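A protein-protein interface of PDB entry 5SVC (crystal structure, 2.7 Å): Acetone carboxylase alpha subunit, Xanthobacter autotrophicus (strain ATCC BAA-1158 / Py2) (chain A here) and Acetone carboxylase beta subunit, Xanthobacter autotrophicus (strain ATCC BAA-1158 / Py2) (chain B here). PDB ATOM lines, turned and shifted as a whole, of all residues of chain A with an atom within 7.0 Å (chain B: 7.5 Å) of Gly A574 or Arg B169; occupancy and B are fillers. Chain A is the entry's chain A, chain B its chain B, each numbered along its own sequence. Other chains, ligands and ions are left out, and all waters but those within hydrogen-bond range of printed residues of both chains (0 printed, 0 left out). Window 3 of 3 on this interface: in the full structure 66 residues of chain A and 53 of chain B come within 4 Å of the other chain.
The side-chain hydroxyl (OG) of Ser A573 sits at hydrogen-bond distance from the backbone carbonyl oxygen (O) of Leu A570 (3.5 Å).
The backbone carbonyl oxygen (O) of Leu A570 sits at hydrogen-bond distance from the backbone NH (N) of Ala A575 (3.1 Å).
The backbone NH of Arg B169 is in hydrogen-bond range of the backbone carbonyl oxygen of Val B155.
The backbone carbonyl oxygen (O) of Ile B166 lies within hydrogen-bond range of the backbone NH (N) of Arg B157, at 2.9 Å.
The backbone carbonyl oxygen of Arg B169 is in hydrogen-bond range of the side-chain hydroxyl of Thr B172 (3.2 Å).
Hydrophobic or aromatic side chains of chain A that line the printed part of chain B: Ile A571 and Ile A577.
Of the 17 printed residues of chain B, 3 touch a printed residue of chain A.
Hydrophobic or aromatic side chains of chain B within 4 Å of the printed part of chain A: Ile B166 and Pro B167.
Among the printed residues, 7 pairs touch across the chains.
Among the printed residues, no Asp or Glu carboxylate lies within 4 Å of a Lys or Arg side-chain nitrogen of the other chain.
O of Leu A570 lies within hydrogen-bond range of NH2 of Arg B169, 3.5 Å away.
The guanidinium group (NH2) of Arg B169 sits at hydrogen-bond distance from the backbone carbonyl oxygen (O) of Ile A571.
The backbone carbonyl oxygen (O) of Gly A574 is in hydrogen-bond range of the guanidinium group (NH1) of Arg B169 (3.5 Å).
O of Ala A575 lies within hydrogen-bond range of NH1 of Arg B169 (2.7 Å).
CG1 of Ile B166 touches CD1 of Ile A571 (3.6 Å).
Pro B167 touches Ile A571.
CG2 of Ile A577 touches NH2 of Arg B169 (3.7 Å).
Printed residues of chain B within 4 Å of Leu A570: Arg B169.
Gly A574 touches just one residue of chain B: Arg B169.
Printed residues of chain A within 4 Å of Pro B167: Ile A571 (3.7 Å).
Arg B169 touches just these residues of chain A: Leu A570 (3.5 Å), Ile A571 (3.3 Å), Gly A574 (3.5 Å), Ala A575 (2.7 Å) and Ile A577 (3.7 Å).
Asp B171 touches none of the printed residues of chain A.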
ATOM      1  N   LEU A 567      -4.954  -5.599  14.335  1.00  0.00           N
ATOM      2  CA  LEU A 567      -4.383  -5.313  15.644  1.00  0.00           C
ATOM      3  C   LEU A 567      -2.875  -5.087  15.603  1.00  0.00           C
ATOM      4  O   LEU A 567      -2.329  -4.460  16.524  1.00  0.00           O
ATOM      5  CB  LEU A 567      -4.754  -6.412  16.646  1.00  0.00           C
ATOM      6  CG  LEU A 567      -5.879  -5.937  17.585  1.00  0.00           C
ATOM      7  CD1 LEU A 567      -6.524  -7.079  18.304  1.00  0.00           C
ATOM      8  CD2 LEU A 567      -5.381  -4.887  18.591  1.00  0.00           C
ATOM      9  N   GLU A 569      -1.467  -3.011  13.497  1.00  0.00           N
ATOM     10  CA  GLU A 569      -1.478  -1.551  13.401  1.00  0.00           C
ATOM     11  C   GLU A 569      -1.976  -0.901  14.685  1.00  0.00           C
ATOM     12  O   GLU A 569      -1.416   0.105  15.131  1.00  0.00           O
ATOM     13  CB  GLU A 569      -2.348  -1.082  12.233  1.00  0.00           C
ATOM     14  CG  GLU A 569      -1.610  -0.436  11.059  1.00  0.00           C
ATOM     15  CD  GLU A 569      -2.567   0.102   9.978  1.00  0.00           C
ATOM     16  OE1 GLU A 569      -3.443   0.940  10.299  1.00  0.00           O
ATOM     17  OE2 GLU A 569      -2.453  -0.327   8.804  1.00  0.00           O
ATOM     18  N   LEU A 570      -3.024  -1.451  15.299  1.00  0.00           N
ATOM     19  CA  LEU A 570      -3.617  -0.780  16.453  1.00  0.00           C
ATOM     20  C   LEU A 570      -2.658  -0.737  17.639  1.00  0.00           C
ATOM     21  O   LEU A 570      -2.491   0.315  18.276  1.00  0.00           O
ATOM     22  CB  LEU A 570      -4.929  -1.459  16.822  1.00  0.00           C
ATOM     23  CG  LEU A 570      -6.056  -1.217  15.827  1.00  0.00           C
ATOM     24  CD1 LEU A 570      -7.271  -1.960  16.332  1.00  0.00           C
ATOM     25  CD2 LEU A 570      -6.345   0.283  15.609  1.00  0.00           C
ATOM     26  N   ILE A 571      -2.020  -1.871  17.950  1.00  0.00           N
ATOM     27  CA  ILE A 571      -0.967  -1.893  18.963  1.00  0.00           C
ATOM     28  C   ILE A 571       0.096  -0.840  18.645  1.00  0.00           C
ATOM     29  O   ILE A 571       0.424   0.010  19.480  1.00  0.00           O
ATOM     30  CB  ILE A 571      -0.347  -3.302  19.042  1.00  0.00           C
ATOM     31  CG1 ILE A 571      -1.361  -4.322  19.563  1.00  0.00           C
ATOM     32  CG2 ILE A 571       0.939  -3.298  19.892  1.00  0.00           C
ATOM     33  CD1 ILE A 571      -0.977  -5.765  19.264  1.00  0.00           C
ATOM     34  N   ALA A 572       0.611  -0.861  17.406  1.00  0.00           N
ATOM     35  CA  ALA A 572       1.757  -0.032  17.002  1.00  0.00           C
ATOM     36  C   ALA A 572       1.436   1.466  16.989  1.00  0.00           C
ATOM     37  O   ALA A 572       2.304   2.292  17.315  1.00  0.00           O
ATOM     38  CB  ALA A 572       2.260  -0.479  15.622  1.00  0.00           C
ATOM     39  N   SER A 573       0.216   1.842  16.600  1.00  0.00           N
ATOM     40  CA  SER A 573      -0.156   3.249  16.481  1.00  0.00           C
ATOM     41  C   SER A 573      -0.667   3.840  17.786  1.00  0.00           C
ATOM     42  O   SER A 573      -1.046   5.009  17.802  1.00  0.00           O
ATOM     43  CB  SER A 573      -1.222   3.438  15.400  1.00  0.00           C
ATOM     44  OG  SER A 573      -2.399   2.725  15.753  1.00  0.00           O
ATOM     45  N   GLY A 574      -0.711   3.069  18.864  1.00  0.00           N
ATOM     46  CA  GLY A 574      -1.138   3.587  20.150  1.00  0.00           C
ATOM     47  C   GLY A 574      -2.632   3.661  20.355  1.00  0.00           C
ATOM     48  O   GLY A 574      -3.068   4.271  21.339  1.00  0.00           O
ATOM     49  N   ALA A 575      -3.426   3.070  19.455  1.00  0.00           N
ATOM     50  CA  ALA A 575      -4.877   3.054  19.571  1.00  0.00           C
ATOM     51  C   ALA A 575      -5.336   2.149  20.720  1.00  0.00           C
ATOM     52  O   ALA A 575      -4.562   1.367  21.282  1.00  0.00           O
ATOM     53  CB  ALA A 575      -5.501   2.579  18.258  1.00  0.00           C
ATOM     54  N   GLU A 576      -6.635   2.233  21.027  1.00  0.00           N
ATOM     55  CA  GLU A 576      -7.266   1.325  21.983  1.00  0.00           C
ATOM     56  C   GLU A 576      -7.156  -0.114  21.500  1.00  0.00           C
ATOM     57  O   GLU A 576      -7.392  -0.394  20.319  1.00  0.00           O
ATOM     58  CB  GLU A 576      -8.748   1.683  22.186  1.00  0.00           C
ATOM     59  CG  GLU A 576      -9.034   2.644  23.353  1.00  0.00           C
ATOM     60  CD  GLU A 576     -10.523   2.906  23.602  1.00  0.00           C
ATOM     61  OE1 GLU A 576     -11.324   2.777  22.654  1.00  0.00           O
ATOM     62  OE2 GLU A 576     -10.891   3.256  24.748  1.00  0.00           O
ATOM     63  N   ILE A 577      -6.765  -1.014  22.406  1.00  0.00           N
ATOM     64  CA  ILE A 577      -6.789  -2.451  22.134  1.00  0.00           C
ATOM     65  C   ILE A 577      -7.602  -3.195  23.195  1.00  0.00           C
ATOM     66  O   ILE A 577      -7.656  -2.797  24.374  1.00  0.00           O
ATOM     67  CB  ILE A 577      -5.370  -3.042  22.023  1.00  0.00           C
ATOM     68  CG1 ILE A 577      -4.594  -2.866  23.316  1.00  0.00           C
ATOM     69  CG2 ILE A 577      -4.605  -2.392  20.899  1.00  0.00           C
ATOM     70  CD1 ILE A 577      -3.211  -3.341  23.203  1.00  0.00           C
ATOM     71  N   ARG B 110      -2.119  -5.081  32.386  1.00  0.00           N
ATOM     72  CA  ARG B 110      -3.493  -4.610  32.303  1.00  0.00           C
ATOM     73  C   ARG B 110      -4.336  -5.648  31.578  1.00  0.00           C
ATOM     74  O   ARG B 110      -3.924  -6.202  30.556  1.00  0.00           O
ATOM     75  CB  ARG B 110      -3.527  -3.248  31.595  1.00  0.00           C
ATOM     76  CG  ARG B 110      -4.902  -2.718  31.081  1.00  0.00           C
ATOM     77  CD  ARG B 110      -5.655  -1.787  32.043  1.00  0.00           C
ATOM     78  NE  ARG B 110      -4.850  -0.659  32.520  1.00  0.00           N
ATOM     79  CZ  ARG B 110      -4.660   0.476  31.848  1.00  0.00           C
ATOM     80  NH1 ARG B 110      -5.207   0.642  30.653  1.00  0.00           N
ATOM     81  NH2 ARG B 110      -3.912   1.446  32.369  1.00  0.00           N
ATOM     82  N   VAL B 154      -0.639  -2.257  33.802  1.00  0.00           N
ATOM     83  CA  VAL B 154       0.029  -1.521  32.735  1.00  0.00           C
ATOM     84  C   VAL B 154      -0.186  -2.277  31.430  1.00  0.00           C
ATOM     85  O   VAL B 154      -0.388  -3.494  31.419  1.00  0.00           O
ATOM     86  CB  VAL B 154       1.534  -1.294  33.006  1.00  0.00           C
ATOM     87  CG1 VAL B 154       1.722  -0.729  34.367  1.00  0.00           C
ATOM     88  CG2 VAL B 154       2.341  -2.539  32.845  1.00  0.00           C
ATOM     89  N   VAL B 155      -0.134  -1.548  30.324  1.00  0.00           N
ATOM     90  CA  VAL B 155      -0.409  -2.096  29.003  1.00  0.00           C
ATOM     91  C   VAL B 155       0.923  -2.461  28.366  1.00  0.00           C
ATOM     92  O   VAL B 155       1.619  -1.606  27.809  1.00  0.00           O
ATOM     93  CB  VAL B 155      -1.184  -1.115  28.137  1.00  0.00           C
ATOM     94  CG1 VAL B 155      -1.494  -1.771  26.800  1.00  0.00           C
ATOM     95  CG2 VAL B 155      -2.442  -0.712  28.872  1.00  0.00           C
ATOM     96  N   GLU B 156       1.282  -3.734  28.471  1.00  0.00           N
ATOM     97  CA  GLU B 156       2.530  -4.254  27.941  1.00  0.00           C
ATOM     98  C   GLU B 156       2.349  -5.754  27.734  1.00  0.00           C
ATOM     99  O   GLU B 156       1.540  -6.387  28.421  1.00  0.00           O
ATOM    100  CB  GLU B 156       3.705  -3.955  28.881  1.00  0.00           C
ATOM    101  CG  GLU B 156       5.045  -4.563  28.432  1.00  0.00           C
ATOM    102  CD  GLU B 156       5.332  -5.986  28.970  1.00  0.00           C
ATOM    103  OE1 GLU B 156       4.547  -6.552  29.773  1.00  0.00           O
ATOM    104  OE2 GLU B 156       6.378  -6.549  28.584  1.00  0.00           O
ATOM    105  N   ARG B 157       3.059  -6.310  26.745  1.00  0.00           N
ATOM    106  CA  ARG B 157       3.008  -7.753  26.529  1.00  0.00           C
ATOM    107  C   ARG B 157       4.287  -8.266  25.875  1.00  0.00           C
ATOM    108  O   ARG B 157       4.645  -7.824  24.775  1.00  0.00           O
ATOM    109  CB  ARG B 157       1.792  -8.110  25.703  1.00  0.00           C
ATOM    110  CG  ARG B 157       1.227  -9.421  26.114  1.00  0.00           C
ATOM    111  CD  ARG B 157       1.288  -9.649  27.628  1.00  0.00           C
ATOM    112  NE  ARG B 157       0.867 -11.027  27.922  1.00  0.00           N
ATOM    113  CZ  ARG B 157       1.616 -12.117  27.783  1.00  0.00           C
ATOM    114  NH1 ARG B 157       2.865 -12.044  27.385  1.00  0.00           N
ATOM    115  NH2 ARG B 157       1.111 -13.290  28.061  1.00  0.00           N
ATOM    116  N   ILE B 166       3.331  -6.330  22.375  1.00  0.00           N
ATOM    117  CA  ILE B 166       2.673  -5.068  22.694  1.00  0.00           C
ATOM    118  C   ILE B 166       3.687  -4.259  23.493  1.00  0.00           C
ATOM    119  O   ILE B 166       3.973  -4.571  24.661  1.00  0.00           O
ATOM    120  CB  ILE B 166       1.356  -5.274  23.466  1.00  0.00           C
ATOM    121  CG1 ILE B 166       0.312  -5.937  22.588  1.00  0.00           C
ATOM    122  CG2 ILE B 166       0.763  -3.959  23.959  1.00  0.00           C
ATOM    123  CD1 ILE B 166      -0.734  -6.642  23.399  1.00  0.00           C
ATOM    124  N   PRO B 167       4.293  -3.252  22.884  1.00  0.00           N
ATOM    125  CA  PRO B 167       5.306  -2.473  23.598  1.00  0.00           C
ATOM    126  C   PRO B 167       4.684  -1.714  24.754  1.00  0.00           C
ATOM    127  O   PRO B 167       3.499  -1.380  24.735  1.00  0.00           O
ATOM    128  CB  PRO B 167       5.851  -1.522  22.526  1.00  0.00           C
ATOM    129  CG  PRO B 167       4.900  -1.644  21.338  1.00  0.00           C
ATOM    130  CD  PRO B 167       4.266  -2.978  21.437  1.00  0.00           C
ATOM    131  N   LEU B 168       5.498  -1.475  25.785  1.00  0.00           N
ATOM    132  CA  LEU B 168       5.017  -0.824  26.998  1.00  0.00           C
ATOM    133  C   LEU B 168       4.559   0.603  26.709  1.00  0.00           C
ATOM    134  O   LEU B 168       5.345   1.455  26.287  1.00  0.00           O
ATOM    135  CB  LEU B 168       6.104  -0.822  28.065  1.00  0.00           C
ATOM    136  CG  LEU B 168       5.823   0.164  29.213  1.00  0.00           C
ATOM    137  CD1 LEU B 168       4.653  -0.240  30.125  1.00  0.00           C
ATOM    138  CD2 LEU B 168       7.082   0.416  30.025  1.00  0.00           C
ATOM    139  N   ARG B 169       3.284   0.866  26.946  1.00  0.00           N
ATOM    140  CA  ARG B 169       2.742   2.213  26.836  1.00  0.00           C
ATOM    141  C   ARG B 169       2.985   2.924  28.163  1.00  0.00           C
ATOM    142  O   ARG B 169       2.134   2.941  29.053  1.00  0.00           O
ATOM    143  CB  ARG B 169       1.273   2.140  26.449  1.00  0.00           C
ATOM    144  CG  ARG B 169       1.053   1.271  25.199  1.00  0.00           C
ATOM    145  CD  ARG B 169      -0.388   1.289  24.777  1.00  0.00           C
ATOM    146  NE  ARG B 169      -0.639   0.609  23.504  1.00  0.00           N
ATOM    147  CZ  ARG B 169      -1.798   0.688  22.849  1.00  0.00           C
ATOM    148  NH1 ARG B 169      -2.768   1.433  23.356  1.00  0.00           N
ATOM    149  NH2 ARG B 169      -1.989   0.040  21.696  1.00  0.00           N
ATOM    150  N   GLU B 170       4.153   3.570  28.266  1.00  0.00           N
ATOM    151  CA  GLU B 170       4.651   4.138  29.525  1.00  0.00           C
ATOM    152  C   GLU B 170       3.663   5.023  30.278  1.00  0.00           C
ATOM    153  O   GLU B 170       3.847   5.247  31.478  1.00  0.00           O
ATOM    154  CB  GLU B 170       5.920   4.958  29.280  1.00  0.00           C
ATOM    155  CG  GLU B 170       7.082   4.145  28.798  1.00  0.00           C
ATOM    156  CD  GLU B 170       8.383   4.825  29.099  1.00  0.00           C
ATOM    157  OE1 GLU B 170       8.343   5.954  29.629  1.00  0.00           O
ATOM    158  OE2 GLU B 170       9.445   4.232  28.824  1.00  0.00           O
ATOM    159  N   ASP B 171       2.657   5.586  29.615  1.00  0.00           N
ATOM    160  CA  ASP B 171       1.716   6.420  30.351  1.00  0.00           C
ATOM    161  C   ASP B 171       0.924   5.603  31.351  1.00  0.00           C
ATOM    162  O   ASP B 171       0.731   6.028  32.496  1.00  0.00           O
ATOM    163  CB  ASP B 171       0.817   7.164  29.388  1.00  0.00           C
ATOM    164  CG  ASP B 171       1.540   8.327  28.763  1.00  0.00           C
ATOM    165  OD1 ASP B 171       2.365   8.962  29.476  1.00  0.00           O
ATOM    166  OD2 ASP B 171       1.318   8.599  27.566  1.00  0.00           O
ATOM    167  N   THR B 172       0.464   4.423  30.940  1.00  0.00           N
ATOM    168  CA  THR B 172      -0.309   3.589  31.845  1.00  0.00           C
ATOM    169  C   THR B 172       0.488   3.199  33.082  1.00  0.00           C
ATOM    170  O   THR B 172      -0.109   2.937  34.135  1.00  0.00           O
ATOM    171  CB  THR B 172      -0.801   2.353  31.105  1.00  0.00           C
ATOM    172  OG1 THR B 172       0.218   1.362  31.116  1.00  0.00           O
ATOM    173  CG2 THR B 172      -1.125   2.702  29.665  1.00  0.00           C
ATOM    174  N   ALA B 173       1.820   3.196  32.987  1.00  0.00           N
ATOM    175  CA  ALA B 173       2.654   2.944  34.158  1.00  0.00           C
ATOM    176  C   ALA B 173       2.663   4.144  35.100  1.00  0.00           C
ATOM    177  O   ALA B 173       2.733   3.977  36.324  1.00  0.00           O
ATOM    178  CB  ALA B 173       4.080   2.575  33.723  1.00  0.00           C
ATOM    179  N   ARG B 174       2.576   5.356  34.560  1.00  0.00           N
ATOM    180  CA  ARG B 174       2.600   6.523  35.427  1.00  0.00           C
ATOM    181  C   ARG B 174       1.295   6.652  36.205  1.00  0.00           C
ATOM    182  O   ARG B 174       1.307   7.037  37.382  1.00  0.00           O
ATOM    183  CB  ARG B 174       2.898   7.771  34.599  1.00  0.00           C
ATOM    184  CG  ARG B 174       4.185   7.639  33.794  1.00  0.00           C
ATOM    185  CD  ARG B 174       4.756   8.989  33.362  1.00  0.00           C
ATOM    186  NE  ARG B 174       6.216   8.933  33.257  1.00  0.00           N
ATOM    187  CZ  ARG B 174       7.053   9.068  34.288  1.00  0.00           C
ATOM    188  NH1 ARG B 174       6.585   9.257  35.519  1.00  0.00           N
ATOM    189  NH2 ARG B 174       8.367   9.007  34.097  1.00  0.00           N
ATOM    190  N   ASN B 201      10.785  -4.260  29.902  1.00  0.00           N
ATOM    191  CA  ASN B 201       9.547  -3.552  30.220  1.00  0.00           C
ATOM    192  C   ASN B 201       9.277  -3.525  31.723  1.00  0.00           C
ATOM    193  O   ASN B 201       8.815  -2.509  32.256  1.00  0.00           O
ATOM    194  CB  ASN B 201       8.391  -4.176  29.462  1.00  0.00           C
ATOM    195  CG  ASN B 201       8.459  -3.895  27.974  1.00  0.00           C
ATOM    196  OD1 ASN B 201       8.811  -2.788  27.547  1.00  0.00           O
ATOM    197  ND2 ASN B 201       8.111  -4.896  27.168  1.00  0.00           N
ATOM    198  N   VAL B 205       8.953  -0.046  33.957  1.00  0.00           N
ATOM    199  CA  VAL B 205       7.843   0.201  34.884  1.00  0.00           C
ATOM    200  C   VAL B 205       8.381   0.540  36.263  1.00  0.00           C
ATOM    201  O   VAL B 205       7.993   1.544  36.872  1.00  0.00           O
ATOM    202  CB  VAL B 205       6.898  -1.015  34.969  1.00  0.00           C
ATOM    203  CG1 VAL B 205       5.864  -0.793  36.073  1.00  0.00           C
ATOM    204  CG2 VAL B 205       6.222  -1.308  33.654  1.00  0.00           C
ATOM    205  N   ILE B 208       9.804   3.939  36.321  1.00  0.00           N
ATOM    206  CA  ILE B 208       8.740   4.945  36.255  1.00  0.00           C
ATOM    207  C   ILE B 208       8.033   5.070  37.595  1.00  0.00           C
ATOM    208  O   ILE B 208       7.742   6.186  38.053  1.00  0.00           O
ATOM    209  CB  ILE B 208       7.745   4.621  35.131  1.00  0.00           C
ATOM    210  CG1 ILE B 208       8.361   4.961  33.773  1.00  0.00           C
ATOM    211  CG2 ILE B 208       6.458   5.395  35.347  1.00  0.00           C
ATOM    212  CD1 ILE B 208       7.643   4.334  32.607  1.00  0.00           C
